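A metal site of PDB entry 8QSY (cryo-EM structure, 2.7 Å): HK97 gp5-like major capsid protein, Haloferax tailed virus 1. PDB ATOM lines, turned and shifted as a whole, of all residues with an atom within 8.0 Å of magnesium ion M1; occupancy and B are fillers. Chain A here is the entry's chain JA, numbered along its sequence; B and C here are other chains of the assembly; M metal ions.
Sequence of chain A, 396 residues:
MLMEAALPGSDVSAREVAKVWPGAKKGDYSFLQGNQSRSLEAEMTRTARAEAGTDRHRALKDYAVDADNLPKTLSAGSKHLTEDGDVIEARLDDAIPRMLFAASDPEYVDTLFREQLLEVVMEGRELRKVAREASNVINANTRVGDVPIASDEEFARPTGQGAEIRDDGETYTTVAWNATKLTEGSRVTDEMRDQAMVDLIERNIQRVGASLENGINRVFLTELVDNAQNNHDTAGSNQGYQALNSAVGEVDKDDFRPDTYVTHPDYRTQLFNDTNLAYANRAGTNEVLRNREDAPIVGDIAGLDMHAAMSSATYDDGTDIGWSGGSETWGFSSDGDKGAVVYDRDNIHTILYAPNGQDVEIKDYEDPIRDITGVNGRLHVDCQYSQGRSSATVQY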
ATOM      1  N   GLU A 153     -25.986  -0.595 -17.531  1.00  0.00           N
ATOM      2  CA  GLU A 153     -25.208  -1.808 -17.736  1.00  0.00           C
ATOM      3  C   GLU A 153     -25.025  -2.563 -16.406  1.00  0.00           C
ATOM      4  O   GLU A 153     -24.688  -1.966 -15.369  1.00  0.00           O
ATOM      5  CB  GLU A 153     -23.844  -1.486 -18.330  1.00  0.00           C
ATOM      6  CG  GLU A 153     -23.883  -1.174 -19.823  1.00  0.00           C
ATOM      7  CD  GLU A 153     -22.523  -0.883 -20.450  1.00  0.00           C
ATOM      8  OE1 GLU A 153     -21.494  -0.951 -19.732  1.00  0.00           O
ATOM      9  OE2 GLU A 153     -22.494  -0.591 -21.653  1.00  0.00           O
ATOM     10  N   GLU A 154     -25.239  -3.884 -16.460  1.00  0.00           N
ATOM     11  CA  GLU A 154     -24.964  -4.797 -15.354  1.00  0.00           C
ATOM     12  C   GLU A 154     -23.827  -5.756 -15.743  1.00  0.00           C
ATOM     13  O   GLU A 154     -23.065  -5.479 -16.676  1.00  0.00           O
ATOM     14  CB  GLU A 154     -26.259  -5.500 -14.924  1.00  0.00           C
ATOM     15  CG  GLU A 154     -27.338  -4.551 -14.423  1.00  0.00           C
ATOM     16  CD  GLU A 154     -28.593  -5.220 -13.900  1.00  0.00           C
ATOM     17  OE1 GLU A 154     -28.502  -6.000 -12.927  1.00  0.00           O
ATOM     18  OE2 GLU A 154     -29.679  -4.960 -14.451  1.00  0.00           O
ATOM     19  N   PHE A 155     -23.731  -6.873 -15.018  1.00  0.00           N
ATOM     20  CA  PHE A 155     -22.715  -7.882 -15.279  1.00  0.00           C
ATOM     21  C   PHE A 155     -23.348  -9.235 -15.584  1.00  0.00           C
ATOM     22  O   PHE A 155     -24.409  -9.592 -15.058  1.00  0.00           O
ATOM     23  CB  PHE A 155     -21.779  -8.016 -14.071  1.00  0.00           C
ATOM     24  CG  PHE A 155     -20.988  -6.772 -13.744  1.00  0.00           C
ATOM     25  CD1 PHE A 155     -21.586  -5.679 -13.105  1.00  0.00           C
ATOM     26  CD2 PHE A 155     -19.640  -6.687 -14.061  1.00  0.00           C
ATOM     27  CE1 PHE A 155     -20.855  -4.537 -12.819  1.00  0.00           C
ATOM     28  CE2 PHE A 155     -18.902  -5.548 -13.769  1.00  0.00           C
ATOM     29  CZ  PHE A 155     -19.506  -4.482 -13.140  1.00  0.00           C
ATOM     30  N   ALA A 156     -22.674  -9.991 -16.458  1.00  0.00           N
ATOM     31  CA  ALA A 156     -22.944 -11.411 -16.627  1.00  0.00           C
ATOM     32  C   ALA A 156     -22.650 -12.140 -15.318  1.00  0.00           C
ATOM     33  O   ALA A 156     -21.964 -11.609 -14.447  1.00  0.00           O
ATOM     34  CB  ALA A 156     -22.074 -11.929 -17.746  1.00  0.00           C
ATOM     35  N   ARG A 157     -23.195 -13.348 -15.144  1.00  0.00           N
ATOM     36  CA  ARG A 157     -22.913 -14.159 -13.963  1.00  0.00           C
ATOM     37  C   ARG A 157     -22.182 -15.433 -14.362  1.00  0.00           C
ATOM     38  O   ARG A 157     -22.348 -15.897 -15.484  1.00  0.00           O
ATOM     39  CB  ARG A 157     -24.194 -14.406 -13.144  1.00  0.00           C
ATOM     40  CG  ARG A 157     -25.247 -15.279 -13.827  1.00  0.00           C
ATOM     41  CD  ARG A 157     -26.200 -15.850 -12.799  1.00  0.00           C
ATOM     42  NE  ARG A 157     -27.347 -15.016 -12.479  1.00  0.00           N
ATOM     43  CZ  ARG A 157     -28.122 -15.156 -11.402  1.00  0.00           C
ATOM     44  NH1 ARG A 157     -29.158 -14.349 -11.230  1.00  0.00           N
ATOM     45  NH2 ARG A 157     -27.872 -16.103 -10.520  1.00  0.00           N
ATOM     46  N   PRO A 158     -21.326 -16.000 -13.476  1.00  0.00           N
ATOM     47  CA  PRO A 158     -20.693 -17.295 -13.724  1.00  0.00           C
ATOM     48  C   PRO A 158     -21.690 -18.449 -13.683  1.00  0.00           C
ATOM     49  O   PRO A 158     -22.569 -18.495 -12.835  1.00  0.00           O
ATOM     50  CB  PRO A 158     -19.659 -17.421 -12.603  1.00  0.00           C
ATOM     51  CG  PRO A 158     -20.149 -16.503 -11.509  1.00  0.00           C
ATOM     52  CD  PRO A 158     -20.888 -15.390 -12.208  1.00  0.00           C
ATOM     53  N   ARG A 166     -29.679 -17.615 -17.340  1.00  0.00           N
ATOM     54  CA  ARG A 166     -30.751 -16.870 -16.696  1.00  0.00           C
ATOM     55  C   ARG A 166     -30.992 -15.515 -17.358  1.00  0.00           C
ATOM     56  O   ARG A 166     -30.081 -14.929 -17.946  1.00  0.00           O
ATOM     57  CB  ARG A 166     -30.440 -16.714 -15.201  1.00  0.00           C
ATOM     58  CG  ARG A 166     -30.512 -18.045 -14.467  1.00  0.00           C
ATOM     59  CD  ARG A 166     -29.996 -17.942 -13.046  1.00  0.00           C
ATOM     60  NE  ARG A 166     -30.290 -19.118 -12.237  1.00  0.00           N
ATOM     61  CZ  ARG A 166     -29.399 -20.008 -11.807  1.00  0.00           C
ATOM     62  NH1 ARG A 166     -29.799 -21.024 -11.073  1.00  0.00           N
ATOM     63  NH2 ARG A 166     -28.105 -19.891 -12.086  1.00  0.00           N
ATOM     64  N   ASP A 167     -32.220 -14.988 -17.223  1.00  0.00           N
ATOM     65  CA  ASP A 167     -32.610 -13.733 -17.843  1.00  0.00           C
ATOM     66  C   ASP A 167     -32.247 -12.515 -16.984  1.00  0.00           C
ATOM     67  O   ASP A 167     -32.739 -12.367 -15.860  1.00  0.00           O
ATOM     68  CB  ASP A 167     -34.111 -13.736 -18.179  1.00  0.00           C
ATOM     69  CG  ASP A 167     -34.581 -14.853 -19.097  1.00  0.00           C
ATOM     70  OD1 ASP A 167     -33.763 -15.338 -19.911  1.00  0.00           O
ATOM     71  OD2 ASP A 167     -35.782 -15.224 -19.020  1.00  0.00           O
ATOM     72  N   ASP A 168     -31.432 -11.612 -17.574  1.00  0.00           N
ATOM     73  CA  ASP A 168     -31.116 -10.271 -17.089  1.00  0.00           C
ATOM     74  C   ASP A 168     -31.410  -9.252 -18.206  1.00  0.00           C
ATOM     75  O   ASP A 168     -30.547  -8.434 -18.559  1.00  0.00           O
ATOM     76  CB  ASP A 168     -29.658 -10.182 -16.604  1.00  0.00           C
ATOM     77  CG  ASP A 168     -29.343 -10.601 -15.173  1.00  0.00           C
ATOM     78  OD1 ASP A 168     -30.275 -10.989 -14.427  1.00  0.00           O
ATOM     79  OD2 ASP A 168     -28.131 -10.501 -14.800  1.00  0.00           O
ATOM     80  N   GLY A 169     -32.635  -9.288 -18.751  1.00  0.00           N
ATOM     81  CA  GLY A 169     -33.023  -8.458 -19.886  1.00  0.00           C
ATOM     82  C   GLY A 169     -33.067  -6.963 -19.573  1.00  0.00           C
ATOM     83  O   GLY A 169     -33.199  -6.575 -18.410  1.00  0.00           O
ATOM     84  N   THR B 183     -22.328 -15.776 -18.431  1.00  0.00           N
ATOM     85  CA  THR B 183     -23.445 -15.711 -19.355  1.00  0.00           C
ATOM     86  C   THR B 183     -24.396 -14.580 -18.993  1.00  0.00           C
ATOM     87  O   THR B 183     -24.524 -14.214 -17.831  1.00  0.00           O
ATOM     88  CB  THR B 183     -24.233 -17.030 -19.415  1.00  0.00           C
ATOM     89  OG1 THR B 183     -24.796 -17.293 -18.129  1.00  0.00           O
ATOM     90  CG2 THR B 183     -23.376 -18.214 -19.813  1.00  0.00           C
ATOM     91  N   GLU B 184     -25.074 -14.050 -20.012  1.00  0.00           N
ATOM     92  CA  GLU B 184     -26.196 -13.135 -19.816  1.00  0.00           C
ATOM     93  C   GLU B 184     -27.258 -13.492 -20.842  1.00  0.00           C
ATOM     94  O   GLU B 184     -26.925 -13.733 -21.996  1.00  0.00           O
ATOM     95  CB  GLU B 184     -25.717 -11.683 -19.992  1.00  0.00           C
ATOM     96  CG  GLU B 184     -26.695 -10.654 -19.446  1.00  0.00           C
ATOM     97  CD  GLU B 184     -26.604 -10.425 -17.951  1.00  0.00           C
ATOM     98  OE1 GLU B 184     -26.529 -11.411 -17.183  1.00  0.00           O
ATOM     99  OE2 GLU B 184     -26.574  -9.240 -17.548  1.00  0.00           O
ATOM    100  N   GLY B 185     -28.535 -13.540 -20.433  1.00  0.00           N
ATOM    101  CA  GLY B 185     -29.608 -13.876 -21.359  1.00  0.00           C
ATOM    102  C   GLY B 185     -30.779 -12.895 -21.285  1.00  0.00           C
ATOM    103  O   GLY B 185     -30.934 -12.149 -20.320  1.00  0.00           O
ATOM    104  N   ARG B 207     -26.781  -4.959 -24.984  1.00  0.00           N
ATOM    105  CA  ARG B 207     -26.766  -5.164 -23.533  1.00  0.00           C
ATOM    106  C   ARG B 207     -25.992  -6.435 -23.146  1.00  0.00           C
ATOM    107  O   ARG B 207     -25.170  -6.392 -22.241  1.00  0.00           O
ATOM    108  CB  ARG B 207     -28.177  -5.207 -22.960  1.00  0.00           C
ATOM    109  CG  ARG B 207     -28.189  -5.589 -21.482  1.00  0.00           C
ATOM    110  CD  ARG B 207     -29.532  -5.467 -20.838  1.00  0.00           C
ATOM    111  NE  ARG B 207     -29.530  -5.938 -19.454  1.00  0.00           N
ATOM    112  CZ  ARG B 207     -29.332  -5.169 -18.387  1.00  0.00           C
ATOM    113  NH1 ARG B 207     -29.359  -5.731 -17.187  1.00  0.00           N
ATOM    114  NH2 ARG B 207     -29.112  -3.875 -18.503  1.00  0.00           N
ATOM    115  N   SER B 211     -22.572  -6.611 -21.076  1.00  0.00           N
ATOM    116  CA  SER B 211     -22.641  -7.362 -19.837  1.00  0.00           C
ATOM    117  C   SER B 211     -21.529  -8.413 -19.736  1.00  0.00           C
ATOM    118  O   SER B 211     -20.954  -8.621 -18.671  1.00  0.00           O
ATOM    119  CB  SER B 211     -24.005  -7.953 -19.708  1.00  0.00           C
ATOM    120  OG  SER B 211     -24.128  -8.687 -18.512  1.00  0.00           O
ATOM    121  N   LEU B 212     -21.169  -9.050 -20.866  1.00  0.00           N
ATOM    122  CA  LEU B 212     -20.026  -9.949 -20.937  1.00  0.00           C
ATOM    123  C   LEU B 212     -18.705  -9.204 -20.801  1.00  0.00           C
ATOM    124  O   LEU B 212     -17.852  -9.665 -20.057  1.00  0.00           O
ATOM    125  CB  LEU B 212     -20.024 -10.742 -22.249  1.00  0.00           C
ATOM    126  CG  LEU B 212     -21.138 -11.759 -22.427  1.00  0.00           C
ATOM    127  CD1 LEU B 212     -21.077 -12.304 -23.833  1.00  0.00           C
ATOM    128  CD2 LEU B 212     -21.044 -12.905 -21.433  1.00  0.00           C
ATOM    129  N   ARG B 218     -14.443  -7.425 -14.485  1.00  0.00           N
ATOM    130  CA  ARG B 218     -14.590  -7.815 -13.082  1.00  0.00           C
ATOM    131  C   ARG B 218     -13.617  -8.930 -12.713  1.00  0.00           C
ATOM    132  O   ARG B 218     -12.978  -8.837 -11.677  1.00  0.00           O
ATOM    133  CB  ARG B 218     -16.041  -8.191 -12.767  1.00  0.00           C
ATOM    134  CG  ARG B 218     -16.216  -8.739 -11.361  1.00  0.00           C
ATOM    135  CD  ARG B 218     -17.675  -8.831 -10.954  1.00  0.00           C
ATOM    136  NE  ARG B 218     -18.211  -7.516 -10.609  1.00  0.00           N
ATOM    137  CZ  ARG B 218     -19.506  -7.229 -10.489  1.00  0.00           C
ATOM    138  NH1 ARG B 218     -19.887  -6.009 -10.161  1.00  0.00           N
ATOM    139  NH2 ARG B 218     -20.411  -8.156 -10.689  1.00  0.00           N
ATOM    140  N   ASP B 320     -23.083  -8.310  -5.787  1.00  0.00           N
ATOM    141  CA  ASP B 320     -23.784  -8.679  -7.013  1.00  0.00           C
ATOM    142  C   ASP B 320     -24.183 -10.157  -6.997  1.00  0.00           C
ATOM    143  O   ASP B 320     -23.517 -10.992  -6.393  1.00  0.00           O
ATOM    144  CB  ASP B 320     -22.948  -8.315  -8.238  1.00  0.00           C
ATOM    145  CG  ASP B 320     -23.748  -8.105  -9.504  1.00  0.00           C
ATOM    146  OD1 ASP B 320     -24.990  -8.267  -9.466  1.00  0.00           O
ATOM    147  OD2 ASP B 320     -23.135  -7.741 -10.522  1.00  0.00           O
ATOM    148  N   ILE B 321     -25.267 -10.491  -7.710  1.00  0.00           N
ATOM    149  CA  ILE B 321     -25.846 -11.834  -7.652  1.00  0.00           C
ATOM    150  C   ILE B 321     -25.002 -12.821  -8.474  1.00  0.00           C
ATOM    151  O   ILE B 321     -24.667 -12.564  -9.624  1.00  0.00           O
ATOM    152  CB  ILE B 321     -27.321 -11.793  -8.065  1.00  0.00           C
ATOM    153  CG1 ILE B 321     -28.128 -10.939  -7.076  1.00  0.00           C
ATOM    154  CG2 ILE B 321     -27.903 -13.191  -8.216  1.00  0.00           C
ATOM    155  CD1 ILE B 321     -29.550 -10.638  -7.493  1.00  0.00           C
ATOM    156  N   TRP B 323     -21.937 -13.643  -7.897  1.00  0.00           N
ATOM    157  CA  TRP B 323     -20.542 -13.318  -7.636  1.00  0.00           C
ATOM    158  C   TRP B 323     -20.243 -13.430  -6.142  1.00  0.00           C
ATOM    159  O   TRP B 323     -21.025 -12.959  -5.313  1.00  0.00           O
ATOM    160  CB  TRP B 323     -20.244 -11.909  -8.155  1.00  0.00           C
ATOM    161  CG  TRP B 323     -20.297 -11.757  -9.646  1.00  0.00           C
ATOM    162  CD1 TRP B 323     -21.387 -11.381 -10.365  1.00  0.00           C
ATOM    163  CD2 TRP B 323     -19.239 -11.992 -10.612  1.00  0.00           C
ATOM    164  NE1 TRP B 323     -21.087 -11.375 -11.704  1.00  0.00           N
ATOM    165  CE2 TRP B 323     -19.781 -11.748 -11.894  1.00  0.00           C
ATOM    166  CE3 TRP B 323     -17.897 -12.381 -10.539  1.00  0.00           C
ATOM    167  CZ2 TRP B 323     -19.018 -11.872 -13.076  1.00  0.00           C
ATOM    168  CZ3 TRP B 323     -17.150 -12.545 -11.689  1.00  0.00           C
ATOM    169  CH2 TRP B 323     -17.712 -12.304 -12.947  1.00  0.00           C
ATOM    170  N   ARG C  79     -37.757 -13.276  -9.064  1.00  0.00           N
ATOM    171  CA  ARG C  79     -37.453 -12.158  -8.193  1.00  0.00           C
ATOM    172  C   ARG C  79     -38.739 -11.741  -7.466  1.00  0.00           C
ATOM    173  O   ARG C  79     -39.704 -11.332  -8.114  1.00  0.00           O
ATOM    174  CB  ARG C  79     -36.929 -10.996  -9.049  1.00  0.00           C
ATOM    175  CG  ARG C  79     -35.466 -11.158  -9.415  1.00  0.00           C
ATOM    176  CD  ARG C  79     -35.084 -10.561 -10.758  1.00  0.00           C
ATOM    177  NE  ARG C  79     -33.700 -10.879 -11.032  1.00  0.00           N
ATOM    178  CZ  ARG C  79     -33.106 -11.109 -12.203  1.00  0.00           C
ATOM    179  NH1 ARG C  79     -31.834 -11.442 -12.179  1.00  0.00           N
ATOM    180  NH2 ARG C  79     -33.753 -10.985 -13.354  1.00  0.00           N
HETATM  181 MG    MG M   1     -26.374 -10.165 -15.351  1.00  0.00          MG
HETATM  182 MG    MG M   2     -30.541  -5.842 -12.820  1.00  0.00          MG
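NE of Arg 207 of chain B sits at hydrogen-bond distance from O of Asp 168.
The side-chain carboxylate (OD1) of Asp 168 lies within salt-bridge range of the guanidinium group (NH1) of Arg 79 of chain C, at 2.8 Å.
The backbone NH (N) of Asp 168 is in hydrogen-bond range of the backbone carbonyl oxygen (O) of Gly 185 of chain B (2.8 Å).
The side-chain carboxylate (OE2) of Glu 184 of chain B lies close to the side-chain hydroxyl (OG) of Ser 211 of chain B, 2.7 Å away.
The backbone NH of Ala 156 lies within hydrogen-bond range of the side-chain hydroxyl of Ser 211 of chain B.
The indole nitrogen (NE1) of Trp 323 of chain B lies within hydrogen-bond range of the backbone carbonyl oxygen (O) of Ala 156 (2.9 Å).
Residues that only touch magnesium ion M1: Ala 156.
Of the 21 residues printed, 4 come within 4 Å of magnesium ion M1.
Along chain A the residues within 4 Å of magnesium ion M1 span positions 155 to 168.
The nearest printed residue that does not touch magnesium ion M1 is Ser 211 of chain B (4.1 Å).
Magnesium ion M1 is bound by the side-chain carboxylate (OD2) of Asp 168, the backbone carbonyl oxygen (O) of Phe 155, the side-chain carboxylate (OE1) of Glu 184 of chain B and the side-chain carboxylate (OE2) of Glu 184 of chain B.
Magnesium ion M1 has four donor atoms within binding distance.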
